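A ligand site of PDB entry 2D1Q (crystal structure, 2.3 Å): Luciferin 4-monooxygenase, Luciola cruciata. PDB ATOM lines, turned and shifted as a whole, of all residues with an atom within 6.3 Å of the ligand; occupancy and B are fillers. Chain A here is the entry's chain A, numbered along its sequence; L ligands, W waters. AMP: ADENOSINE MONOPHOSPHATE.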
ATOM      1  N   ASN A 199      23.429 -12.631  -0.435  1.00  0.00           N
ATOM      2  CA  ASN A 199      22.870 -11.927  -1.578  1.00  0.00           C
ATOM      3  C   ASN A 199      23.858 -12.059  -2.731  1.00  0.00           C
ATOM      4  O   ASN A 199      25.071 -11.889  -2.526  1.00  0.00           O
ATOM      5  CB  ASN A 199      22.681 -10.431  -1.262  1.00  0.00           C
ATOM      6  CG  ASN A 199      21.720 -10.159  -0.111  1.00  0.00           C
ATOM      7  OD1 ASN A 199      21.899  -9.182   0.605  1.00  0.00           O
ATOM      8  ND2 ASN A 199      20.709 -10.996   0.069  1.00  0.00           N
ATOM      9  N   SER A 200      23.361 -12.314  -3.940  1.00  0.00           N
ATOM     10  CA  SER A 200      24.235 -12.210  -5.130  1.00  0.00           C
ATOM     11  C   SER A 200      24.560 -10.750  -5.524  1.00  0.00           C
ATOM     12  O   SER A 200      24.007  -9.804  -4.937  1.00  0.00           O
ATOM     13  CB  SER A 200      23.630 -12.979  -6.322  1.00  0.00           C
ATOM     14  OG  SER A 200      22.368 -12.447  -6.680  1.00  0.00           O
ATOM     15  N   SER A 201      25.446 -10.586  -6.522  1.00  0.00           N
ATOM     16  CA  SER A 201      25.857  -9.266  -7.030  1.00  0.00           C
ATOM     17  C   SER A 201      25.016  -8.748  -8.204  1.00  0.00           C
ATOM     18  O   SER A 201      24.025  -9.387  -8.630  1.00  0.00           O
ATOM     19  CB  SER A 201      27.317  -9.299  -7.464  1.00  0.00           C
ATOM     20  OG  SER A 201      27.465 -10.162  -8.587  1.00  0.00           O
ATOM     21  N   HIS A 247      30.062 -10.918   0.007  1.00  0.00           N
ATOM     22  CA  HIS A 247      29.707 -11.780  -1.095  1.00  0.00           C
ATOM     23  C   HIS A 247      30.402 -13.149  -0.951  1.00  0.00           C
ATOM     24  O   HIS A 247      31.505 -13.231  -0.377  1.00  0.00           O
ATOM     25  CB  HIS A 247      30.125 -11.087  -2.392  1.00  0.00           C
ATOM     26  CG  HIS A 247      29.643 -11.783  -3.623  1.00  0.00           C
ATOM     27  ND1 HIS A 247      30.364 -12.796  -4.240  1.00  0.00           N
ATOM     28  CD2 HIS A 247      28.511 -11.624  -4.350  1.00  0.00           C
ATOM     29  CE1 HIS A 247      29.691 -13.230  -5.285  1.00  0.00           C
ATOM     30  NE2 HIS A 247      28.565 -12.536  -5.386  1.00  0.00           N
ATOM     31  N   SER A 316      41.575 -15.625  -9.919  1.00  0.00           N
ATOM     32  CA  SER A 316      40.478 -14.763 -10.357  1.00  0.00           C
ATOM     33  C   SER A 316      39.135 -15.494 -10.305  1.00  0.00           C
ATOM     34  O   SER A 316      39.073 -16.741 -10.306  1.00  0.00           O
ATOM     35  CB  SER A 316      40.731 -14.247 -11.773  1.00  0.00           C
ATOM     36  OG  SER A 316      39.660 -13.434 -12.234  1.00  0.00           O
ATOM     37  N   GLY A 317      38.066 -14.718 -10.240  1.00  0.00           N
ATOM     38  CA  GLY A 317      36.716 -15.258 -10.274  1.00  0.00           C
ATOM     39  C   GLY A 317      35.695 -14.143 -10.364  1.00  0.00           C
ATOM     40  O   GLY A 317      36.060 -12.956 -10.391  1.00  0.00           O
ATOM     41  N   GLY A 318      34.420 -14.531 -10.413  1.00  0.00           N
ATOM     42  CA  GLY A 318      33.335 -13.594 -10.255  1.00  0.00           C
ATOM     43  C   GLY A 318      32.659 -13.167 -11.527  1.00  0.00           C
ATOM     44  O   GLY A 318      31.463 -12.876 -11.533  1.00  0.00           O
ATOM     45  N   ALA A 319      33.440 -13.133 -12.618  1.00  0.00           N
ATOM     46  CA  ALA A 319      33.044 -12.529 -13.874  1.00  0.00           C
ATOM     47  C   ALA A 319      33.959 -13.070 -14.963  1.00  0.00           C
ATOM     48  O   ALA A 319      35.063 -13.545 -14.655  1.00  0.00           O
ATOM     49  CB  ALA A 319      33.166 -10.990 -13.785  1.00  0.00           C
ATOM     50  N   PRO A 320      33.551 -13.007 -16.234  1.00  0.00           N
ATOM     51  CA  PRO A 320      34.373 -13.558 -17.318  1.00  0.00           C
ATOM     52  C   PRO A 320      35.748 -12.890 -17.352  1.00  0.00           C
ATOM     53  O   PRO A 320      35.887 -11.691 -17.109  1.00  0.00           O
ATOM     54  CB  PRO A 320      33.571 -13.211 -18.581  1.00  0.00           C
ATOM     55  CG  PRO A 320      32.174 -12.993 -18.092  1.00  0.00           C
ATOM     56  CD  PRO A 320      32.298 -12.400 -16.729  1.00  0.00           C
ATOM     57  N   LEU A 321      36.791 -13.675 -17.602  1.00  0.00           N
ATOM     58  CA  LEU A 321      38.109 -13.082 -17.687  1.00  0.00           C
ATOM     59  C   LEU A 321      38.661 -13.263 -19.101  1.00  0.00           C
ATOM     60  O   LEU A 321      38.733 -14.373 -19.615  1.00  0.00           O
ATOM     61  CB  LEU A 321      39.062 -13.648 -16.635  1.00  0.00           C
ATOM     62  CG  LEU A 321      40.578 -13.419 -16.811  1.00  0.00           C
ATOM     63  CD1 LEU A 321      40.925 -11.920 -16.744  1.00  0.00           C
ATOM     64  CD2 LEU A 321      41.419 -14.230 -15.806  1.00  0.00           C
ATOM     65  N   GLN A 340      41.635 -19.882 -11.918  1.00  0.00           N
ATOM     66  CA  GLN A 340      40.258 -19.398 -11.927  1.00  0.00           C
ATOM     67  C   GLN A 340      39.391 -20.274 -11.039  1.00  0.00           C
ATOM     68  O   GLN A 340      39.668 -21.462 -10.866  1.00  0.00           O
ATOM     69  CB  GLN A 340      39.681 -19.409 -13.334  1.00  0.00           C
ATOM     70  CG  GLN A 340      40.171 -18.271 -14.204  1.00  0.00           C
ATOM     71  CD  GLN A 340      39.185 -17.921 -15.304  1.00  0.00           C
ATOM     72  OE1 GLN A 340      38.070 -17.430 -15.026  1.00  0.00           O
ATOM     73  NE2 GLN A 340      39.582 -18.149 -16.549  1.00  0.00           N
ATOM     74  N   GLY A 341      38.377 -19.658 -10.446  1.00  0.00           N
ATOM     75  CA  GLY A 341      37.255 -20.361  -9.833  1.00  0.00           C
ATOM     76  C   GLY A 341      35.974 -19.847 -10.485  1.00  0.00           C
ATOM     77  O   GLY A 341      35.897 -18.678 -10.861  1.00  0.00           O
ATOM     78  N   TYR A 342      34.987 -20.727 -10.644  1.00  0.00           N
ATOM     79  CA  TYR A 342      33.632 -20.359 -11.065  1.00  0.00           C
ATOM     80  C   TYR A 342      32.572 -21.004 -10.160  1.00  0.00           C
ATOM     81  O   TYR A 342      32.647 -22.196  -9.850  1.00  0.00           O
ATOM     82  CB  TYR A 342      33.388 -20.781 -12.514  1.00  0.00           C
ATOM     83  CG  TYR A 342      31.925 -20.932 -12.869  1.00  0.00           C
ATOM     84  CD1 TYR A 342      31.304 -22.198 -12.843  1.00  0.00           C
ATOM     85  CD2 TYR A 342      31.158 -19.829 -13.234  1.00  0.00           C
ATOM     86  CE1 TYR A 342      29.953 -22.343 -13.163  1.00  0.00           C
ATOM     87  CE2 TYR A 342      29.827 -19.964 -13.563  1.00  0.00           C
ATOM     88  CZ  TYR A 342      29.227 -21.231 -13.533  1.00  0.00           C
ATOM     89  OH  TYR A 342      27.903 -21.355 -13.868  1.00  0.00           O
ATOM     90  N   GLY A 343      31.602 -20.196  -9.752  1.00  0.00           N
ATOM     91  CA  GLY A 343      30.454 -20.642  -9.007  1.00  0.00           C
ATOM     92  C   GLY A 343      29.410 -19.549  -8.902  1.00  0.00           C
ATOM     93  O   GLY A 343      29.557 -18.486  -9.523  1.00  0.00           O
ATOM     94  N   LEU A 344      28.370 -19.802  -8.093  1.00  0.00           N
ATOM     95  CA  LEU A 344      27.240 -18.904  -7.947  1.00  0.00           C
ATOM     96  C   LEU A 344      27.062 -18.764  -6.469  1.00  0.00           C
ATOM     97  O   LEU A 344      27.551 -19.613  -5.735  1.00  0.00           O
ATOM     98  CB  LEU A 344      25.954 -19.532  -8.546  1.00  0.00           C
ATOM     99  CG  LEU A 344      25.783 -19.545 -10.061  1.00  0.00           C
ATOM    100  CD1 LEU A 344      26.633 -20.655 -10.729  1.00  0.00           C
ATOM    101  CD2 LEU A 344      24.296 -19.684 -10.433  1.00  0.00           C
ATOM    102  N   THR A 345      26.374 -17.701  -6.023  1.00  0.00           N
ATOM    103  CA  THR A 345      25.921 -17.621  -4.621  1.00  0.00           C
ATOM    104  C   THR A 345      25.151 -18.901  -4.180  1.00  0.00           C
ATOM    105  O   THR A 345      25.408 -19.455  -3.100  1.00  0.00           O
ATOM    106  CB  THR A 345      25.056 -16.371  -4.402  1.00  0.00           C
ATOM    107  OG1 THR A 345      25.868 -15.193  -4.558  1.00  0.00           O
ATOM    108  CG2 THR A 345      24.622 -16.284  -2.973  1.00  0.00           C
ATOM    109  N   GLU A 346      24.220 -19.334  -5.030  1.00  0.00           N
ATOM    110  CA  GLU A 346      23.419 -20.554  -4.858  1.00  0.00           C
ATOM    111  C   GLU A 346      24.168 -21.907  -4.684  1.00  0.00           C
ATOM    112  O   GLU A 346      23.577 -22.874  -4.176  1.00  0.00           O
ATOM    113  CB  GLU A 346      22.399 -20.640  -6.016  1.00  0.00           C
ATOM    114  CG  GLU A 346      21.331 -19.545  -5.929  1.00  0.00           C
ATOM    115  CD  GLU A 346      21.710 -18.235  -6.613  1.00  0.00           C
ATOM    116  OE1 GLU A 346      22.898 -18.041  -6.990  1.00  0.00           O
ATOM    117  OE2 GLU A 346      20.800 -17.404  -6.787  1.00  0.00           O
ATOM    118  N   SER A 364      37.984 -22.136 -16.867  1.00  0.00           N
ATOM    119  CA  SER A 364      37.614 -21.885 -15.472  1.00  0.00           C
ATOM    120  C   SER A 364      38.041 -23.031 -14.589  1.00  0.00           C
ATOM    121  O   SER A 364      38.063 -22.895 -13.363  1.00  0.00           O
ATOM    122  CB  SER A 364      36.112 -21.638 -15.324  1.00  0.00           C
ATOM    123  OG  SER A 364      35.847 -20.241 -15.203  1.00  0.00           O
ATOM    124  N   THR A 422      22.379 -22.886 -13.930  1.00  0.00           N
ATOM    125  CA  THR A 422      23.176 -21.713 -13.582  1.00  0.00           C
ATOM    126  C   THR A 422      22.696 -20.435 -14.277  1.00  0.00           C
ATOM    127  O   THR A 422      22.870 -19.329 -13.740  1.00  0.00           O
ATOM    128  CB  THR A 422      24.660 -21.940 -13.904  1.00  0.00           C
ATOM    129  OG1 THR A 422      24.822 -22.199 -15.307  1.00  0.00           O
ATOM    130  CG2 THR A 422      25.204 -23.208 -13.210  1.00  0.00           C
ATOM    131  N   GLY A 423      22.076 -20.584 -15.441  1.00  0.00           N
ATOM    132  CA  GLY A 423      21.783 -19.442 -16.286  1.00  0.00           C
ATOM    133  C   GLY A 423      23.068 -18.963 -16.975  1.00  0.00           C
ATOM    134  O   GLY A 423      23.084 -17.884 -17.554  1.00  0.00           O
ATOM    135  N   ASP A 424      24.131 -19.772 -16.922  1.00  0.00           N
ATOM    136  CA  ASP A 424      25.410 -19.450 -17.556  1.00  0.00           C
ATOM    137  C   ASP A 424      25.619 -20.315 -18.760  1.00  0.00           C
ATOM    138  O   ASP A 424      25.272 -21.490 -18.755  1.00  0.00           O
ATOM    139  CB  ASP A 424      26.584 -19.656 -16.589  1.00  0.00           C
ATOM    140  CG  ASP A 424      26.568 -18.677 -15.429  1.00  0.00           C
ATOM    141  OD1 ASP A 424      26.296 -17.491 -15.675  1.00  0.00           O
ATOM    142  OD2 ASP A 424      26.803 -19.011 -14.242  1.00  0.00           O
ATOM    143  N   ILE A 436      33.716 -21.009 -19.311  1.00  0.00           N
ATOM    144  CA  ILE A 436      32.482 -20.263 -19.060  1.00  0.00           C
ATOM    145  C   ILE A 436      32.488 -19.027 -19.958  1.00  0.00           C
ATOM    146  O   ILE A 436      33.472 -18.268 -19.977  1.00  0.00           O
ATOM    147  CB  ILE A 436      32.297 -19.939 -17.518  1.00  0.00           C
ATOM    148  CG1 ILE A 436      32.376 -21.220 -16.673  1.00  0.00           C
ATOM    149  CG2 ILE A 436      30.964 -19.293 -17.264  1.00  0.00           C
ATOM    150  CD1 ILE A 436      31.283 -22.273 -16.994  1.00  0.00           C
ATOM    151  N   VAL A 437      31.428 -18.844 -20.729  1.00  0.00           N
ATOM    152  CA  VAL A 437      31.457 -17.842 -21.785  1.00  0.00           C
ATOM    153  C   VAL A 437      30.836 -16.523 -21.299  1.00  0.00           C
ATOM    154  O   VAL A 437      31.482 -15.469 -21.316  1.00  0.00           O
ATOM    155  CB  VAL A 437      30.804 -18.366 -23.102  1.00  0.00           C
ATOM    156  CG1 VAL A 437      30.773 -17.272 -24.168  1.00  0.00           C
ATOM    157  CG2 VAL A 437      31.531 -19.600 -23.637  1.00  0.00           C
ATOM    158  N   ASP A 438      29.605 -16.607 -20.817  1.00  0.00           N
ATOM    159  CA  ASP A 438      28.833 -15.450 -20.399  1.00  0.00           C
ATOM    160  C   ASP A 438      27.503 -15.905 -19.830  1.00  0.00           C
ATOM    161  O   ASP A 438      27.204 -17.104 -19.791  1.00  0.00           O
ATOM    162  CB  ASP A 438      28.588 -14.523 -21.583  1.00  0.00           C
ATOM    163  CG  ASP A 438      28.616 -13.067 -21.195  1.00  0.00           C
ATOM    164  OD1 ASP A 438      28.110 -12.730 -20.108  1.00  0.00           O
ATOM    165  OD2 ASP A 438      29.118 -12.203 -21.946  1.00  0.00           O
ATOM    166  N   ARG A 439      26.704 -14.944 -19.365  1.00  0.00           N
ATOM    167  CA  ARG A 439      25.362 -15.210 -18.873  1.00  0.00           C
ATOM    168  C   ARG A 439      24.374 -15.313 -20.060  1.00  0.00           C
ATOM    169  O   ARG A 439      24.409 -14.488 -20.979  1.00  0.00           O
ATOM    170  CB  ARG A 439      24.904 -14.090 -17.958  1.00  0.00           C
ATOM    171  CG  ARG A 439      25.581 -14.054 -16.599  1.00  0.00           C
ATOM    172  CD  ARG A 439      25.274 -12.779 -15.817  1.00  0.00           C
ATOM    173  NE  ARG A 439      26.011 -11.664 -16.401  1.00  0.00           N
ATOM    174  CZ  ARG A 439      25.784 -10.371 -16.160  1.00  0.00           C
ATOM    175  NH1 ARG A 439      24.843  -9.984 -15.322  1.00  0.00           N
ATOM    176  NH2 ARG A 439      26.540  -9.464 -16.777  1.00  0.00           N
ATOM    177  N   THR A 529      31.415  -7.768  -7.940  1.00  0.00           N
ATOM    178  CA  THR A 529      32.331  -8.853  -8.291  1.00  0.00           C
ATOM    179  C   THR A 529      32.781  -8.816  -9.759  1.00  0.00           C
ATOM    180  O   THR A 529      33.406  -9.753 -10.240  1.00  0.00           O
ATOM    181  CB  THR A 529      31.730 -10.228  -7.921  1.00  0.00           C
ATOM    182  OG1 THR A 529      30.410 -10.337  -8.478  1.00  0.00           O
ATOM    183  CG2 THR A 529      31.530 -10.313  -6.407  1.00  0.00           C
ATOM    184  N   LYS A 531      30.656  -8.176 -12.584  1.00  0.00           N
ATOM    185  CA  LYS A 531      29.665  -8.424 -13.649  1.00  0.00           C
ATOM    186  C   LYS A 531      29.063  -7.121 -14.195  1.00  0.00           C
ATOM    187  O   LYS A 531      28.627  -6.246 -13.439  1.00  0.00           O
ATOM    188  CB  LYS A 531      28.581  -9.426 -13.240  1.00  0.00           C
ATOM    189  CG  LYS A 531      29.090 -10.849 -13.054  1.00  0.00           C
ATOM    190  CD  LYS A 531      28.026 -11.788 -12.497  1.00  0.00           C
ATOM    191  CE  LYS A 531      27.200 -11.170 -11.384  1.00  0.00           C
ATOM    192  NZ  LYS A 531      25.742 -11.416 -11.607  1.00  0.00           N
HETATM  193  P   AMP L   1      26.527 -14.149  -8.229  1.00  0.00           P
HETATM  194  O1P AMP L   1      26.282 -15.157  -7.186  1.00  0.00           O
HETATM  195  O2P AMP L   1      25.223 -13.973  -9.009  1.00  0.00           O
HETATM  196  O3P AMP L   1      26.904 -12.802  -7.601  1.00  0.00           O
HETATM  197  O5' AMP L   1      27.688 -14.570  -9.231  1.00  0.00           O
HETATM  198  C5' AMP L   1      27.598 -15.779  -9.942  1.00  0.00           C
HETATM  199  C4' AMP L   1      27.795 -15.498 -11.412  1.00  0.00           C
HETATM  200  O4' AMP L   1      29.015 -14.822 -11.689  1.00  0.00           O
HETATM  201  C3' AMP L   1      27.814 -16.762 -12.260  1.00  0.00           C
HETATM  202  O3' AMP L   1      26.495 -17.191 -12.573  1.00  0.00           O
HETATM  203  C2' AMP L   1      28.543 -16.290 -13.496  1.00  0.00           C
HETATM  204  O2' AMP L   1      27.591 -15.602 -14.283  1.00  0.00           O
HETATM  205  C1' AMP L   1      29.536 -15.273 -12.927  1.00  0.00           C
HETATM  206  N9  AMP L   1      30.855 -15.909 -12.726  1.00  0.00           N
HETATM  207  C8  AMP L   1      31.399 -16.337 -11.528  1.00  0.00           C
HETATM  208  N7  AMP L   1      32.625 -16.852 -11.774  1.00  0.00           N
HETATM  209  C5  AMP L   1      32.879 -16.777 -13.110  1.00  0.00           C
HETATM  210  C6  AMP L   1      33.965 -17.172 -13.890  1.00  0.00           C
HETATM  211  N6  AMP L   1      35.032 -17.753 -13.344  1.00  0.00           N
HETATM  212  N1  AMP L   1      33.920 -16.970 -15.262  1.00  0.00           N
HETATM  213  C2  AMP L   1      32.812 -16.395 -15.838  1.00  0.00           C
HETATM  214  N3  AMP L   1      31.757 -16.012 -15.049  1.00  0.00           N
HETATM  215  C4  AMP L   1      31.768 -16.199 -13.714  1.00  0.00           C
HETATM  216  O   HOH W   1      36.161 -16.962 -17.038  1.00  0.00           O
HETATM  217  O   HOH W   2      30.177 -12.984  -9.372  1.00  0.00           O
HETATM  218  O   HOH W   3      29.504 -14.895 -16.624  1.00  0.00           O
HETATM  219  O   HOH W   4      23.803 -16.423 -14.605  1.00  0.00           O
HETATM  220  O   HOH W   5      23.909 -16.052  -8.673  1.00  0.00           O
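Merely in contact with the ligand: Ser 200, Gly 343, Arg 439, Pro 320, Tyr 342, Leu 344, Ala 319 and Ile 436. Hydrophobic or aromatic side chains that line the ligand: His 247, Tyr 342, Leu 344 and Ile 436. Within 4 Å of the ligand: Ser 200, Ser 201, His 247, Gly 318, Ala 319, Pro 320, Gln 340, Gly 341, Tyr 342, Gly 343, Leu 344, Thr 345, Ser 364, Asp 424, Ile 436, Arg 439 and Lys 531.
The backbone NH (N) of Thr 345 is in hydrogen-bond range of an oxygen (O1P) of the ligand (2.8 Å). An oxygen (O3P) of the ligand is in hydrogen-bond range of the side-chain hydroxyl (OG) of Ser 201. The backbone carbonyl oxygen of Gly 341 lies within hydrogen-bond range of a nitrogen (N6) of the ligand (2.8 Å). NE2 of His 247 is in hydrogen-bond range of O3P of the ligand, 2.8 Å away. The backbone NH (N) of Gly 318 is in hydrogen-bond range of a nitrogen (N7) of the ligand (3.2 Å). A nitrogen (N6) of the ligand is in hydrogen-bond range of the side-chain hydroxyl of Ser 364, at 3.2 Å. The side-chain hydroxyl (OG1) of Thr 345 lies within hydrogen-bond range of an oxygen (O1P) of the ligand, at 2.7 Å. The side-chain carboxylate (OD2) of Asp 424 lies within hydrogen-bond range of an oxygen (O3') of the ligand (2.5 Å). A nitrogen (N6) of the ligand is in hydrogen-bond range of the side-chain amide oxygen of Gln 340 (3.5 Å). The side-chain amino group of Lys 531 is in salt-bridge range of an oxygen (O2P) of the ligand (3.7 Å). An oxygen (O3P) of the ligand sits at hydrogen-bond distance from the backbone NH (N) of Ser 201, at 2.9 Å.
Water W5 bridges O2P of the ligand (2.5 Å) and OE1 of Glu 346 (2.8 Å). Water W1 lies within hydrogen-bond range of the side-chain amide oxygen (OE1) of Gln 340, a nitrogen (N1) of the ligand and the backbone NH (N) of Leu 321. Water W2 lies within hydrogen-bond range of O of Gly 318 (2.5 Å), OG1 of Thr 529 (2.8 Å) and O5' of the ligand (3.0 Å).
N of Gly 341 is in hydrogen-bond range of O of Ser 316 (3.0 Å). OH of Tyr 342 is in hydrogen-bond range of OD2 of Asp 424 (2.6 Å). OG1 of Thr 529 lies within hydrogen-bond range of OG of Ser 201 (3.0 Å). The backbone NH (N) of Asp 424 sits at hydrogen-bond distance from the side-chain hydroxyl (OG1) of Thr 422, at 3.0 Å.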
